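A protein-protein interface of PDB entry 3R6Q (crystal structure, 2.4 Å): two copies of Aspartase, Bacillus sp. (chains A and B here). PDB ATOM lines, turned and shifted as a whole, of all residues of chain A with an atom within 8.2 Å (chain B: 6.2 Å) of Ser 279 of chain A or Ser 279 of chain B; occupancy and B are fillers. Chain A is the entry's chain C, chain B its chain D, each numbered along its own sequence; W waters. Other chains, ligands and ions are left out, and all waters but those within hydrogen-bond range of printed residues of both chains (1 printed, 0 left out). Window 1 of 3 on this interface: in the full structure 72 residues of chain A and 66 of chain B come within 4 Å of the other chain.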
ATOM      1  N   ASP A 211     -17.399   9.647  30.608  1.00  0.00           N
ATOM      2  CA  ASP A 211     -18.250  10.164  29.538  1.00  0.00           C
ATOM      3  C   ASP A 211     -17.573  11.242  28.695  1.00  0.00           C
ATOM      4  O   ASP A 211     -17.757  11.288  27.472  1.00  0.00           O
ATOM      5  CB  ASP A 211     -19.544  10.722  30.129  1.00  0.00           C
ATOM      6  CG  ASP A 211     -20.411   9.640  30.772  1.00  0.00           C
ATOM      7  OD1 ASP A 211     -20.453   8.499  30.240  1.00  0.00           O
ATOM      8  OD2 ASP A 211     -21.054   9.931  31.808  1.00  0.00           O
ATOM      9  N   ARG A 214     -15.202   9.617  26.397  1.00  0.00           N
ATOM     10  CA  ARG A 214     -15.919   8.892  25.330  1.00  0.00           C
ATOM     11  C   ARG A 214     -16.488   9.834  24.278  1.00  0.00           C
ATOM     12  O   ARG A 214     -16.360   9.582  23.083  1.00  0.00           O
ATOM     13  CB  ARG A 214     -17.052   7.995  25.873  1.00  0.00           C
ATOM     14  CG  ARG A 214     -16.633   6.693  26.550  1.00  0.00           C
ATOM     15  CD  ARG A 214     -17.875   5.863  26.924  1.00  0.00           C
ATOM     16  NE  ARG A 214     -18.596   6.440  28.055  1.00  0.00           N
ATOM     17  CZ  ARG A 214     -18.472   6.026  29.314  1.00  0.00           C
ATOM     18  NH1 ARG A 214     -17.672   5.000  29.604  1.00  0.00           N
ATOM     19  NH2 ARG A 214     -19.148   6.631  30.286  1.00  0.00           N
ATOM     20  N   ILE A 215     -17.141  10.900  24.732  1.00  0.00           N
ATOM     21  CA  ILE A 215     -17.680  11.928  23.846  1.00  0.00           C
ATOM     22  C   ILE A 215     -16.553  12.595  23.030  1.00  0.00           C
ATOM     23  O   ILE A 215     -16.673  12.773  21.812  1.00  0.00           O
ATOM     24  CB  ILE A 215     -18.500  12.979  24.652  1.00  0.00           C
ATOM     25  CG1 ILE A 215     -19.693  12.298  25.334  1.00  0.00           C
ATOM     26  CG2 ILE A 215     -18.972  14.122  23.753  1.00  0.00           C
ATOM     27  CD1 ILE A 215     -20.602  13.233  26.122  1.00  0.00           C
ATOM     28  N   THR A 218     -15.269  10.582  19.981  1.00  0.00           N
ATOM     29  CA  THR A 218     -16.155  10.503  18.840  1.00  0.00           C
ATOM     30  C   THR A 218     -15.912  11.649  17.877  1.00  0.00           C
ATOM     31  O   THR A 218     -16.434  11.630  16.774  1.00  0.00           O
ATOM     32  CB  THR A 218     -17.651  10.434  19.237  1.00  0.00           C
ATOM     33  OG1 THR A 218     -18.102  11.716  19.699  1.00  0.00           O
ATOM     34  CG2 THR A 218     -17.869   9.346  20.305  1.00  0.00           C
ATOM     35  N   ASP A 272     -21.714   5.857  10.161  1.00  0.00           N
ATOM     36  CA  ASP A 272     -21.280   5.377  11.495  1.00  0.00           C
ATOM     37  C   ASP A 272     -20.653   6.449  12.394  1.00  0.00           C
ATOM     38  O   ASP A 272     -20.714   6.346  13.607  1.00  0.00           O
ATOM     39  CB  ASP A 272     -20.309   4.188  11.373  1.00  0.00           C
ATOM     40  CG  ASP A 272     -19.130   4.496  10.465  1.00  0.00           C
ATOM     41  OD1 ASP A 272     -19.388   4.969   9.332  1.00  0.00           O
ATOM     42  OD2 ASP A 272     -17.956   4.280  10.867  1.00  0.00           O
ATOM     43  N   CYS A 273     -20.033   7.468  11.818  1.00  0.00           N
ATOM     44  CA  CYS A 273     -19.548   8.569  12.641  1.00  0.00           C
ATOM     45  C   CYS A 273     -20.702   9.273  13.388  1.00  0.00           C
ATOM     46  O   CYS A 273     -20.517   9.757  14.510  1.00  0.00           O
ATOM     47  CB  CYS A 273     -18.742   9.569  11.808  1.00  0.00           C
ATOM     48  SG  CYS A 273     -19.713  10.346  10.514  1.00  0.00           S
ATOM     49  N   TYR A 274     -21.886   9.318  12.778  1.00  0.00           N
ATOM     50  CA  TYR A 274     -23.057   9.908  13.451  1.00  0.00           C
ATOM     51  C   TYR A 274     -23.604   9.047  14.590  1.00  0.00           C
ATOM     52  O   TYR A 274     -23.900   9.577  15.665  1.00  0.00           O
ATOM     53  CB  TYR A 274     -24.170  10.205  12.454  1.00  0.00           C
ATOM     54  CG  TYR A 274     -23.704  11.027  11.277  1.00  0.00           C
ATOM     55  CD1 TYR A 274     -23.679  10.483   9.997  1.00  0.00           C
ATOM     56  CD2 TYR A 274     -23.276  12.340  11.449  1.00  0.00           C
ATOM     57  CE1 TYR A 274     -23.237  11.220   8.918  1.00  0.00           C
ATOM     58  CE2 TYR A 274     -22.837  13.088  10.372  1.00  0.00           C
ATOM     59  CZ  TYR A 274     -22.823  12.518   9.110  1.00  0.00           C
ATOM     60  OH  TYR A 274     -22.399  13.258   8.035  1.00  0.00           O
ATOM     61  N   THR A 275     -23.755   7.739  14.357  1.00  0.00           N
ATOM     62  CA  THR A 275     -24.223   6.833  15.398  1.00  0.00           C
ATOM     63  C   THR A 275     -23.158   6.644  16.480  1.00  0.00           C
ATOM     64  O   THR A 275     -23.474   6.342  17.631  1.00  0.00           O
ATOM     65  CB  THR A 275     -24.635   5.458  14.846  1.00  0.00           C
ATOM     66  OG1 THR A 275     -23.589   4.931  14.024  1.00  0.00           O
ATOM     67  CG2 THR A 275     -25.885   5.569  14.020  1.00  0.00           C
ATOM     68  N   GLU A 276     -21.893   6.828  16.118  1.00  0.00           N
ATOM     69  CA  GLU A 276     -20.827   6.770  17.113  1.00  0.00           C
ATOM     70  C   GLU A 276     -21.002   7.886  18.135  1.00  0.00           C
ATOM     71  O   GLU A 276     -20.831   7.654  19.322  1.00  0.00           O
ATOM     72  CB  GLU A 276     -19.452   6.864  16.476  1.00  0.00           C
ATOM     73  CG  GLU A 276     -18.340   6.546  17.450  1.00  0.00           C
ATOM     74  CD  GLU A 276     -16.960   6.799  16.890  1.00  0.00           C
ATOM     75  OE1 GLU A 276     -16.046   7.133  17.666  1.00  0.00           O
ATOM     76  OE2 GLU A 276     -16.783   6.653  15.674  1.00  0.00           O
ATOM     77  N   VAL A 277     -21.358   9.085  17.674  1.00  0.00           N
ATOM     78  CA  VAL A 277     -21.630  10.220  18.571  1.00  0.00           C
ATOM     79  C   VAL A 277     -22.847   9.980  19.462  1.00  0.00           C
ATOM     80  O   VAL A 277     -22.736  10.081  20.676  1.00  0.00           O
ATOM     81  CB  VAL A 277     -21.789  11.571  17.802  1.00  0.00           C
ATOM     82  CG1 VAL A 277     -22.068  12.707  18.758  1.00  0.00           C
ATOM     83  CG2 VAL A 277     -20.536  11.879  16.996  1.00  0.00           C
ATOM     84  N   SER A 278     -23.997   9.672  18.872  1.00  0.00           N
ATOM     85  CA  SER A 278     -25.216   9.471  19.644  1.00  0.00           C
ATOM     86  C   SER A 278     -25.062   8.455  20.773  1.00  0.00           C
ATOM     87  O   SER A 278     -25.627   8.648  21.866  1.00  0.00           O
ATOM     88  CB  SER A 278     -26.364   9.051  18.739  1.00  0.00           C
ATOM     89  OG  SER A 278     -27.554   8.831  19.482  1.00  0.00           O
ATOM     90  N   SER A 279     -24.316   7.380  20.504  1.00  0.00           N
ATOM     91  CA  SER A 279     -24.087   6.301  21.460  1.00  0.00           C
ATOM     92  C   SER A 279     -23.382   6.809  22.724  1.00  0.00           C
ATOM     93  O   SER A 279     -23.817   6.521  23.844  1.00  0.00           O
ATOM     94  CB  SER A 279     -23.268   5.176  20.811  1.00  0.00           C
ATOM     95  OG  SER A 279     -23.974   4.585  19.729  1.00  0.00           O
ATOM     96  N   ALA A 280     -22.302   7.571  22.526  1.00  0.00           N
ATOM     97  CA  ALA A 280     -21.557   8.191  23.628  1.00  0.00           C
ATOM     98  C   ALA A 280     -22.400   9.199  24.415  1.00  0.00           C
ATOM     99  O   ALA A 280     -22.172   9.388  25.613  1.00  0.00           O
ATOM    100  CB  ALA A 280     -20.245   8.837  23.124  1.00  0.00           C
ATOM    101  N   LEU A 281     -23.370   9.828  23.745  1.00  0.00           N
ATOM    102  CA  LEU A 281     -24.307  10.738  24.414  1.00  0.00           C
ATOM    103  C   LEU A 281     -25.401   9.958  25.152  1.00  0.00           C
ATOM    104  O   LEU A 281     -25.895  10.419  26.189  1.00  0.00           O
ATOM    105  CB  LEU A 281     -24.950  11.728  23.442  1.00  0.00           C
ATOM    106  CG  LEU A 281     -24.135  12.651  22.521  1.00  0.00           C
ATOM    107  CD1 LEU A 281     -25.073  13.451  21.631  1.00  0.00           C
ATOM    108  CD2 LEU A 281     -23.223  13.580  23.282  1.00  0.00           C
ATOM    109  N   LYS A 282     -25.775   8.789  24.610  1.00  0.00           N
ATOM    110  CA  LYS A 282     -26.723   7.891  25.266  1.00  0.00           C
ATOM    111  C   LYS A 282     -26.108   7.391  26.557  1.00  0.00           C
ATOM    112  O   LYS A 282     -26.740   7.474  27.603  1.00  0.00           O
ATOM    113  CB  LYS A 282     -27.080   6.706  24.368  1.00  0.00           C
ATOM    114  CG  LYS A 282     -28.192   5.803  24.896  1.00  0.00           C
ATOM    115  CD  LYS A 282     -27.860   4.317  24.728  1.00  0.00           C
ATOM    116  CE  LYS A 282     -27.363   3.943  23.331  1.00  0.00           C
ATOM    117  NZ  LYS A 282     -26.669   2.585  23.226  1.00  0.00           N
ATOM    118  N   VAL A 283     -24.869   6.904  26.494  1.00  0.00           N
ATOM    119  CA  VAL A 283     -24.188   6.369  27.684  1.00  0.00           C
ATOM    120  C   VAL A 283     -24.081   7.417  28.783  1.00  0.00           C
ATOM    121  O   VAL A 283     -24.384   7.157  29.957  1.00  0.00           O
ATOM    122  CB  VAL A 283     -22.776   5.868  27.356  1.00  0.00           C
ATOM    123  CG1 VAL A 283     -22.017   5.519  28.652  1.00  0.00           C
ATOM    124  CG2 VAL A 283     -22.847   4.654  26.412  1.00  0.00           C
ATOM    125  N   CYS A 284     -23.629   8.608  28.393  1.00  0.00           N
ATOM    126  CA  CYS A 284     -23.570   9.737  29.283  1.00  0.00           C
ATOM    127  C   CYS A 284     -24.893  10.024  30.000  1.00  0.00           C
ATOM    128  O   CYS A 284     -24.900  10.338  31.182  1.00  0.00           O
ATOM    129  CB  CYS A 284     -23.143  10.972  28.505  1.00  0.00           C
ATOM    130  SG  CYS A 284     -23.082  12.427  29.514  1.00  0.00           S
ATOM    131  N   MET A 285     -26.008   9.929  29.307  1.00  0.00           N
ATOM    132  CA  MET A 285     -27.276  10.273  29.946  1.00  0.00           C
ATOM    133  C   MET A 285     -27.839   9.147  30.840  1.00  0.00           C
ATOM    134  O   MET A 285     -28.664   9.400  31.728  1.00  0.00           O
ATOM    135  CB  MET A 285     -28.294  10.782  28.926  1.00  0.00           C
ATOM    136  CG  MET A 285     -27.946  12.149  28.338  1.00  0.00           C
ATOM    137  SD  MET A 285     -27.595  13.454  29.564  1.00  0.00           S
ATOM    138  CE  MET A 285     -29.075  13.459  30.574  1.00  0.00           C
ATOM    139  N   ILE A 286     -27.366   7.920  30.623  1.00  0.00           N
ATOM    140  CA  ILE A 286     -27.712   6.808  31.505  1.00  0.00           C
ATOM    141  C   ILE A 286     -27.163   7.033  32.918  1.00  0.00           C
ATOM    142  O   ILE A 286     -27.838   6.763  33.930  1.00  0.00           O
ATOM    143  CB  ILE A 286     -27.221   5.465  30.935  1.00  0.00           C
ATOM    144  CG1 ILE A 286     -27.905   5.176  29.594  1.00  0.00           C
ATOM    145  CG2 ILE A 286     -27.515   4.331  31.905  1.00  0.00           C
ATOM    146  CD1 ILE A 286     -27.142   4.226  28.712  1.00  0.00           C
ATOM    147  N   VAL A 340     -32.854  11.905  24.962  1.00  0.00           N
ATOM    148  CA  VAL A 340     -31.657  11.382  24.317  1.00  0.00           C
ATOM    149  C   VAL A 340     -31.784   9.886  24.020  1.00  0.00           C
ATOM    150  O   VAL A 340     -31.327   9.451  22.956  1.00  0.00           O
ATOM    151  CB  VAL A 340     -30.396  11.657  25.151  1.00  0.00           C
ATOM    152  CG1 VAL A 340     -29.190  11.087  24.471  1.00  0.00           C
ATOM    153  CG2 VAL A 340     -30.221  13.152  25.346  1.00  0.00           C
ATOM    154  N   ASP A 344     -31.744   8.469  20.247  1.00  0.00           N
ATOM    155  CA  ASP A 344     -30.710   7.529  19.829  1.00  0.00           C
ATOM    156  C   ASP A 344     -31.293   6.363  19.011  1.00  0.00           C
ATOM    157  O   ASP A 344     -30.636   5.857  18.092  1.00  0.00           O
ATOM    158  CB  ASP A 344     -29.880   7.015  21.002  1.00  0.00           C
ATOM    159  CG  ASP A 344     -28.893   5.937  20.578  1.00  0.00           C
ATOM    160  OD1 ASP A 344     -29.112   4.751  20.942  1.00  0.00           O
ATOM    161  OD2 ASP A 344     -27.927   6.262  19.839  1.00  0.00           O
ATOM    162  N   ILE A 347     -31.913   7.822  15.560  1.00  0.00           N
ATOM    163  CA  ILE A 347     -30.630   7.876  14.858  1.00  0.00           C
ATOM    164  C   ILE A 347     -30.268   6.478  14.318  1.00  0.00           C
ATOM    165  O   ILE A 347     -29.898   6.329  13.153  1.00  0.00           O
ATOM    166  CB  ILE A 347     -29.562   8.458  15.801  1.00  0.00           C
ATOM    167  CG1 ILE A 347     -29.729   9.985  15.873  1.00  0.00           C
ATOM    168  CG2 ILE A 347     -28.172   8.079  15.364  1.00  0.00           C
ATOM    169  CD1 ILE A 347     -29.153  10.654  17.091  1.00  0.00           C
ATOM    170  N   THR A 348     -30.445   5.459  15.167  1.00  0.00           N
ATOM    171  CA  THR A 348     -30.182   4.069  14.821  1.00  0.00           C
ATOM    172  C   THR A 348     -30.992   3.650  13.589  1.00  0.00           C
ATOM    173  O   THR A 348     -30.421   3.201  12.594  1.00  0.00           O
ATOM    174  CB  THR A 348     -30.508   3.157  16.009  1.00  0.00           C
ATOM    175  OG1 THR A 348     -29.586   3.416  17.071  1.00  0.00           O
ATOM    176  CG2 THR A 348     -30.428   1.700  15.640  1.00  0.00           C
ATOM    177  N   LEU A 369     -29.445  14.368  16.349  1.00  0.00           N
ATOM    178  CA  LEU A 369     -28.081  14.416  16.888  1.00  0.00           C
ATOM    179  C   LEU A 369     -27.798  15.830  17.422  1.00  0.00           C
ATOM    180  O   LEU A 369     -27.342  16.006  18.561  1.00  0.00           O
ATOM    181  CB  LEU A 369     -27.077  14.012  15.808  1.00  0.00           C
ATOM    182  CG  LEU A 369     -25.641  13.832  16.274  1.00  0.00           C
ATOM    183  CD1 LEU A 369     -25.539  12.609  17.175  1.00  0.00           C
ATOM    184  CD2 LEU A 369     -24.747  13.710  15.063  1.00  0.00           C
ATOM    185  N   TYR B 274     -20.297  -1.392  30.621  1.00  0.00           N
ATOM    186  CA  TYR B 274     -21.181  -2.314  29.890  1.00  0.00           C
ATOM    187  C   TYR B 274     -21.978  -1.662  28.771  1.00  0.00           C
ATOM    188  O   TYR B 274     -22.053  -2.203  27.673  1.00  0.00           O
ATOM    189  CB  TYR B 274     -22.123  -3.079  30.826  1.00  0.00           C
ATOM    190  CG  TYR B 274     -21.420  -3.686  32.002  1.00  0.00           C
ATOM    191  CD1 TYR B 274     -21.556  -3.137  33.273  1.00  0.00           C
ATOM    192  CD2 TYR B 274     -20.581  -4.789  31.841  1.00  0.00           C
ATOM    193  CE1 TYR B 274     -20.880  -3.679  34.359  1.00  0.00           C
ATOM    194  CE2 TYR B 274     -19.908  -5.331  32.920  1.00  0.00           C
ATOM    195  CZ  TYR B 274     -20.058  -4.771  34.172  1.00  0.00           C
ATOM    196  OH  TYR B 274     -19.405  -5.327  35.248  1.00  0.00           O
ATOM    197  N   THR B 275     -22.586  -0.515  29.052  1.00  0.00           N
ATOM    198  CA  THR B 275     -23.324   0.240  28.054  1.00  0.00           C
ATOM    199  C   THR B 275     -22.408   0.735  26.934  1.00  0.00           C
ATOM    200  O   THR B 275     -22.832   0.878  25.777  1.00  0.00           O
ATOM    201  CB  THR B 275     -24.062   1.434  28.703  1.00  0.00           C
ATOM    202  OG1 THR B 275     -23.130   2.258  29.419  1.00  0.00           O
ATOM    203  CG2 THR B 275     -25.128   0.924  29.687  1.00  0.00           C
ATOM    204  N   GLU B 276     -21.147   0.987  27.273  1.00  0.00           N
ATOM    205  CA  GLU B 276     -20.164   1.415  26.279  1.00  0.00           C
ATOM    206  C   GLU B 276     -19.903   0.259  25.296  1.00  0.00           C
ATOM    207  O   GLU B 276     -19.947   0.456  24.077  1.00  0.00           O
ATOM    208  CB  GLU B 276     -18.873   1.910  26.960  1.00  0.00           C
ATOM    209  CG  GLU B 276     -17.753   2.356  26.037  1.00  0.00           C
ATOM    210  CD  GLU B 276     -16.426   2.596  26.779  1.00  0.00           C
ATOM    211  OE1 GLU B 276     -15.360   2.461  26.135  1.00  0.00           O
ATOM    212  OE2 GLU B 276     -16.434   2.915  27.997  1.00  0.00           O
ATOM    213  N   VAL B 277     -19.670  -0.943  25.822  1.00  0.00           N
ATOM    214  CA  VAL B 277     -19.446  -2.119  24.963  1.00  0.00           C
ATOM    215  C   VAL B 277     -20.635  -2.365  24.043  1.00  0.00           C
ATOM    216  O   VAL B 277     -20.442  -2.572  22.854  1.00  0.00           O
ATOM    217  CB  VAL B 277     -19.151  -3.388  25.783  1.00  0.00           C
ATOM    218  CG1 VAL B 277     -19.025  -4.638  24.881  1.00  0.00           C
ATOM    219  CG2 VAL B 277     -17.890  -3.197  26.625  1.00  0.00           C
ATOM    220  N   SER B 278     -21.853  -2.302  24.596  1.00  0.00           N
ATOM    221  CA  SER B 278     -23.096  -2.569  23.862  1.00  0.00           C
ATOM    222  C   SER B 278     -23.364  -1.571  22.742  1.00  0.00           C
ATOM    223  O   SER B 278     -23.763  -1.961  21.636  1.00  0.00           O
ATOM    224  CB  SER B 278     -24.285  -2.598  24.821  1.00  0.00           C
ATOM    225  OG  SER B 278     -25.517  -2.638  24.115  1.00  0.00           O
ATOM    226  N   SER B 279     -23.138  -0.289  23.030  1.00  0.00           N
ATOM    227  CA  SER B 279     -23.224   0.765  22.020  1.00  0.00           C
ATOM    228  C   SER B 279     -22.327   0.505  20.819  1.00  0.00           C
ATOM    229  O   SER B 279     -22.730   0.747  19.672  1.00  0.00           O
ATOM    230  CB  SER B 279     -22.875   2.121  22.633  1.00  0.00           C
ATOM    231  OG  SER B 279     -23.747   2.396  23.716  1.00  0.00           O
ATOM    232  N   ALA B 280     -21.116   0.008  21.075  1.00  0.00           N
ATOM    233  CA  ALA B 280     -20.167  -0.277  19.995  1.00  0.00           C
ATOM    234  C   ALA B 280     -20.617  -1.497  19.163  1.00  0.00           C
ATOM    235  O   ALA B 280     -20.405  -1.544  17.942  1.00  0.00           O
ATOM    236  CB  ALA B 280     -18.782  -0.459  20.550  1.00  0.00           C
ATOM    237  N   LEU B 281     -21.262  -2.466  19.820  1.00  0.00           N
ATOM    238  CA  LEU B 281     -21.843  -3.624  19.124  1.00  0.00           C
ATOM    239  C   LEU B 281     -23.037  -3.214  18.273  1.00  0.00           C
ATOM    240  O   LEU B 281     -23.248  -3.757  17.190  1.00  0.00           O
ATOM    241  CB  LEU B 281     -22.293  -4.712  20.114  1.00  0.00           C
ATOM    242  CG  LEU B 281     -21.297  -5.251  21.127  1.00  0.00           C
ATOM    243  CD1 LEU B 281     -21.913  -6.399  21.879  1.00  0.00           C
ATOM    244  CD2 LEU B 281     -19.978  -5.666  20.477  1.00  0.00           C
ATOM    245  N   LYS B 282     -23.813  -2.259  18.779  1.00  0.00           N
ATOM    246  CA  LYS B 282     -25.023  -1.795  18.115  1.00  0.00           C
ATOM    247  C   LYS B 282     -24.678  -1.039  16.831  1.00  0.00           C
ATOM    248  O   LYS B 282     -25.182  -1.358  15.747  1.00  0.00           O
ATOM    249  CB  LYS B 282     -25.843  -0.937  19.080  1.00  0.00           C
ATOM    250  CG  LYS B 282     -27.252  -0.580  18.572  1.00  0.00           C
ATOM    251  CD  LYS B 282     -27.383   0.907  18.415  1.00  0.00           C
ATOM    252  CE  LYS B 282     -27.749   1.562  19.721  1.00  0.00           C
ATOM    253  NZ  LYS B 282     -27.128   2.933  19.844  1.00  0.00           N
ATOM    254  N   VAL B 283     -23.794  -0.053  16.956  1.00  0.00           N
ATOM    255  CA  VAL B 283     -23.245   0.671  15.805  1.00  0.00           C
ATOM    256  C   VAL B 283     -22.693  -0.288  14.740  1.00  0.00           C
ATOM    257  O   VAL B 283     -22.989  -0.154  13.552  1.00  0.00           O
ATOM    258  CB  VAL B 283     -22.186   1.694  16.272  1.00  0.00           C
ATOM    259  CG1 VAL B 283     -21.414   2.299  15.080  1.00  0.00           C
ATOM    260  CG2 VAL B 283     -22.868   2.790  17.111  1.00  0.00           C
ATOM    261  N   CYS B 284     -21.933  -1.287  15.173  1.00  0.00           N
ATOM    262  CA  CYS B 284     -21.410  -2.279  14.251  1.00  0.00           C
ATOM    263  C   CYS B 284     -22.534  -2.973  13.488  1.00  0.00           C
ATOM    264  O   CYS B 284     -22.440  -3.133  12.270  1.00  0.00           O
ATOM    265  CB  CYS B 284     -20.532  -3.285  14.994  1.00  0.00           C
ATOM    266  SG  CYS B 284     -19.942  -4.655  13.997  1.00  0.00           S
ATOM    267  N   ASP B 344     -29.592  -3.917  23.192  1.00  0.00           N
ATOM    268  CA  ASP B 344     -29.022  -2.660  23.637  1.00  0.00           C
ATOM    269  C   ASP B 344     -30.000  -1.766  24.426  1.00  0.00           C
ATOM    270  O   ASP B 344     -29.556  -1.016  25.279  1.00  0.00           O
ATOM    271  CB  ASP B 344     -28.416  -1.871  22.462  1.00  0.00           C
ATOM    272  CG  ASP B 344     -27.861  -0.540  22.900  1.00  0.00           C
ATOM    273  OD1 ASP B 344     -28.525   0.490  22.650  1.00  0.00           O
ATOM    274  OD2 ASP B 344     -26.796  -0.539  23.558  1.00  0.00           O
HETATM  275  O   HOH W   1     -26.553   0.796  26.031  1.00  0.00           O
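Thr 275 of chain A touches Val 283 of chain B (OG1 to CG1, 3.6 Å). Ser 279 of chain A touches Ser 279 of chain B. NZ of Lys 282 of chain B touches OG of Ser 279 of chain A, 3.6 Å away. Val 283 of chain B touches Ser 279 of chain A (CG2 to OG, 3.4 Å). Val 283 of chain A touches Thr 275 of chain B. Val 283 of chain A touches Ser 279 of chain B (CG2 to OG, 3.6 Å). Thr 275 of chain B touches Ile 286 of chain A (CG2 to CD1, 3.99 Å). Lys 282 of chain B touches Thr 348 of chain A.
Of the printed residues of chain B, Arg 214 of chain A touches Glu 276. Ser 279 of chain A touches just these residues of chain B: Ser 279 (3.6 Å), Lys 282 (3.6 Å) and Val 283 (3.4 Å). Of the printed residues of chain A, Thr 275 of chain B touches Val 283 (3.5 Å) and Ile 286 (3.99 Å). No residue of chain A comes within 4 Å of Ser 278 of chain B. Ser 279 of chain B touches just these residues of chain A: Ser 279 (3.6 Å), Lys 282 (3.0 Å) and Val 283 (3.6 Å). No residue of chain A comes within 4 Å of Ala 280 of chain B. Printed residues of chain A within 4 Å of Val 283 of chain B: Thr 275 (3.6 Å) and Ser 279 (3.4 Å).
Thr 275 of chain A touches Val 283 of chain B, and with the chains exchanged Val 283 of chain A touches Thr 275 of chain B. Ser 279 of chain A touches Lys 282 of chain B, and with the chains exchanged Lys 282 of chain A touches Ser 279 of chain B. Ser 279 of chain A touches Val 283 of chain B, and with the chains exchanged Val 283 of chain A touches Ser 279 of chain B. Lys 282 of chain A touches its own counterpart, Lys 282 of chain B. Of the 13 pairs that touch across the chains among the printed residues, 10 have their exchanged pair printed and touching as well.
The guanidinium group (NH1) of Arg 214 of chain A lies within salt-bridge range of the side-chain carboxylate (OE2) of Glu 276 of chain B (2.9 Å). The side-chain amino group (NZ) of Lys 282 of chain A sits at hydrogen-bond distance from the side-chain hydroxyl (OG) of Ser 279 of chain B, 3.0 Å away. The side-chain amino group (NZ) of Lys 282 of chain A is in salt-bridge range of the side-chain carboxylate (OD1) of Asp 344 of chain B. NZ of Lys 282 of chain B lies within salt-bridge range of OD1 of Asp 344 of chain A (2.9 Å). NZ of Lys 282 of chain B sits close to NZ of Lys 282 of chain A, 3.4 Å away.
The backbone carbonyl oxygen of Thr 275 of chain A lies within hydrogen-bond range of the side-chain hydroxyl of Ser 279 of chain A, 2.8 Å away. OG of Ser 278 of chain A sits at hydrogen-bond distance from OD2 of Asp 344 of chain A, 2.6 Å away. NZ of Lys 282 of chain A is in salt-bridge range of OD1 of Asp 344 of chain A, at 3.98 Å. The side-chain hydroxyl (OG1) of Thr 348 of chain A lies within hydrogen-bond range of the backbone carbonyl oxygen (O) of Asp 344 of chain A (2.8 Å). The side-chain hydroxyl of Ser 279 of chain B lies within hydrogen-bond range of the backbone carbonyl oxygen of Thr 275 of chain B, at 2.7 Å. The side-chain amino group (NZ) of Lys 282 of chain B is in salt-bridge range of the side-chain carboxylate (OD1) of Asp 344 of chain B, 3.97 Å away.
Of the 12 printed residues of chain B, 6 touch a printed residue of chain A. Hydrophobic or aromatic side chains of chain A that line the printed part of chain B: Val 283 and Ile 286. Among the printed residues, 13 pairs touch across the chains.
Water W1 bridges the side-chain carboxylate of Asp 344 of chain B and the side-chain amino group of Lys 282 of chain A.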
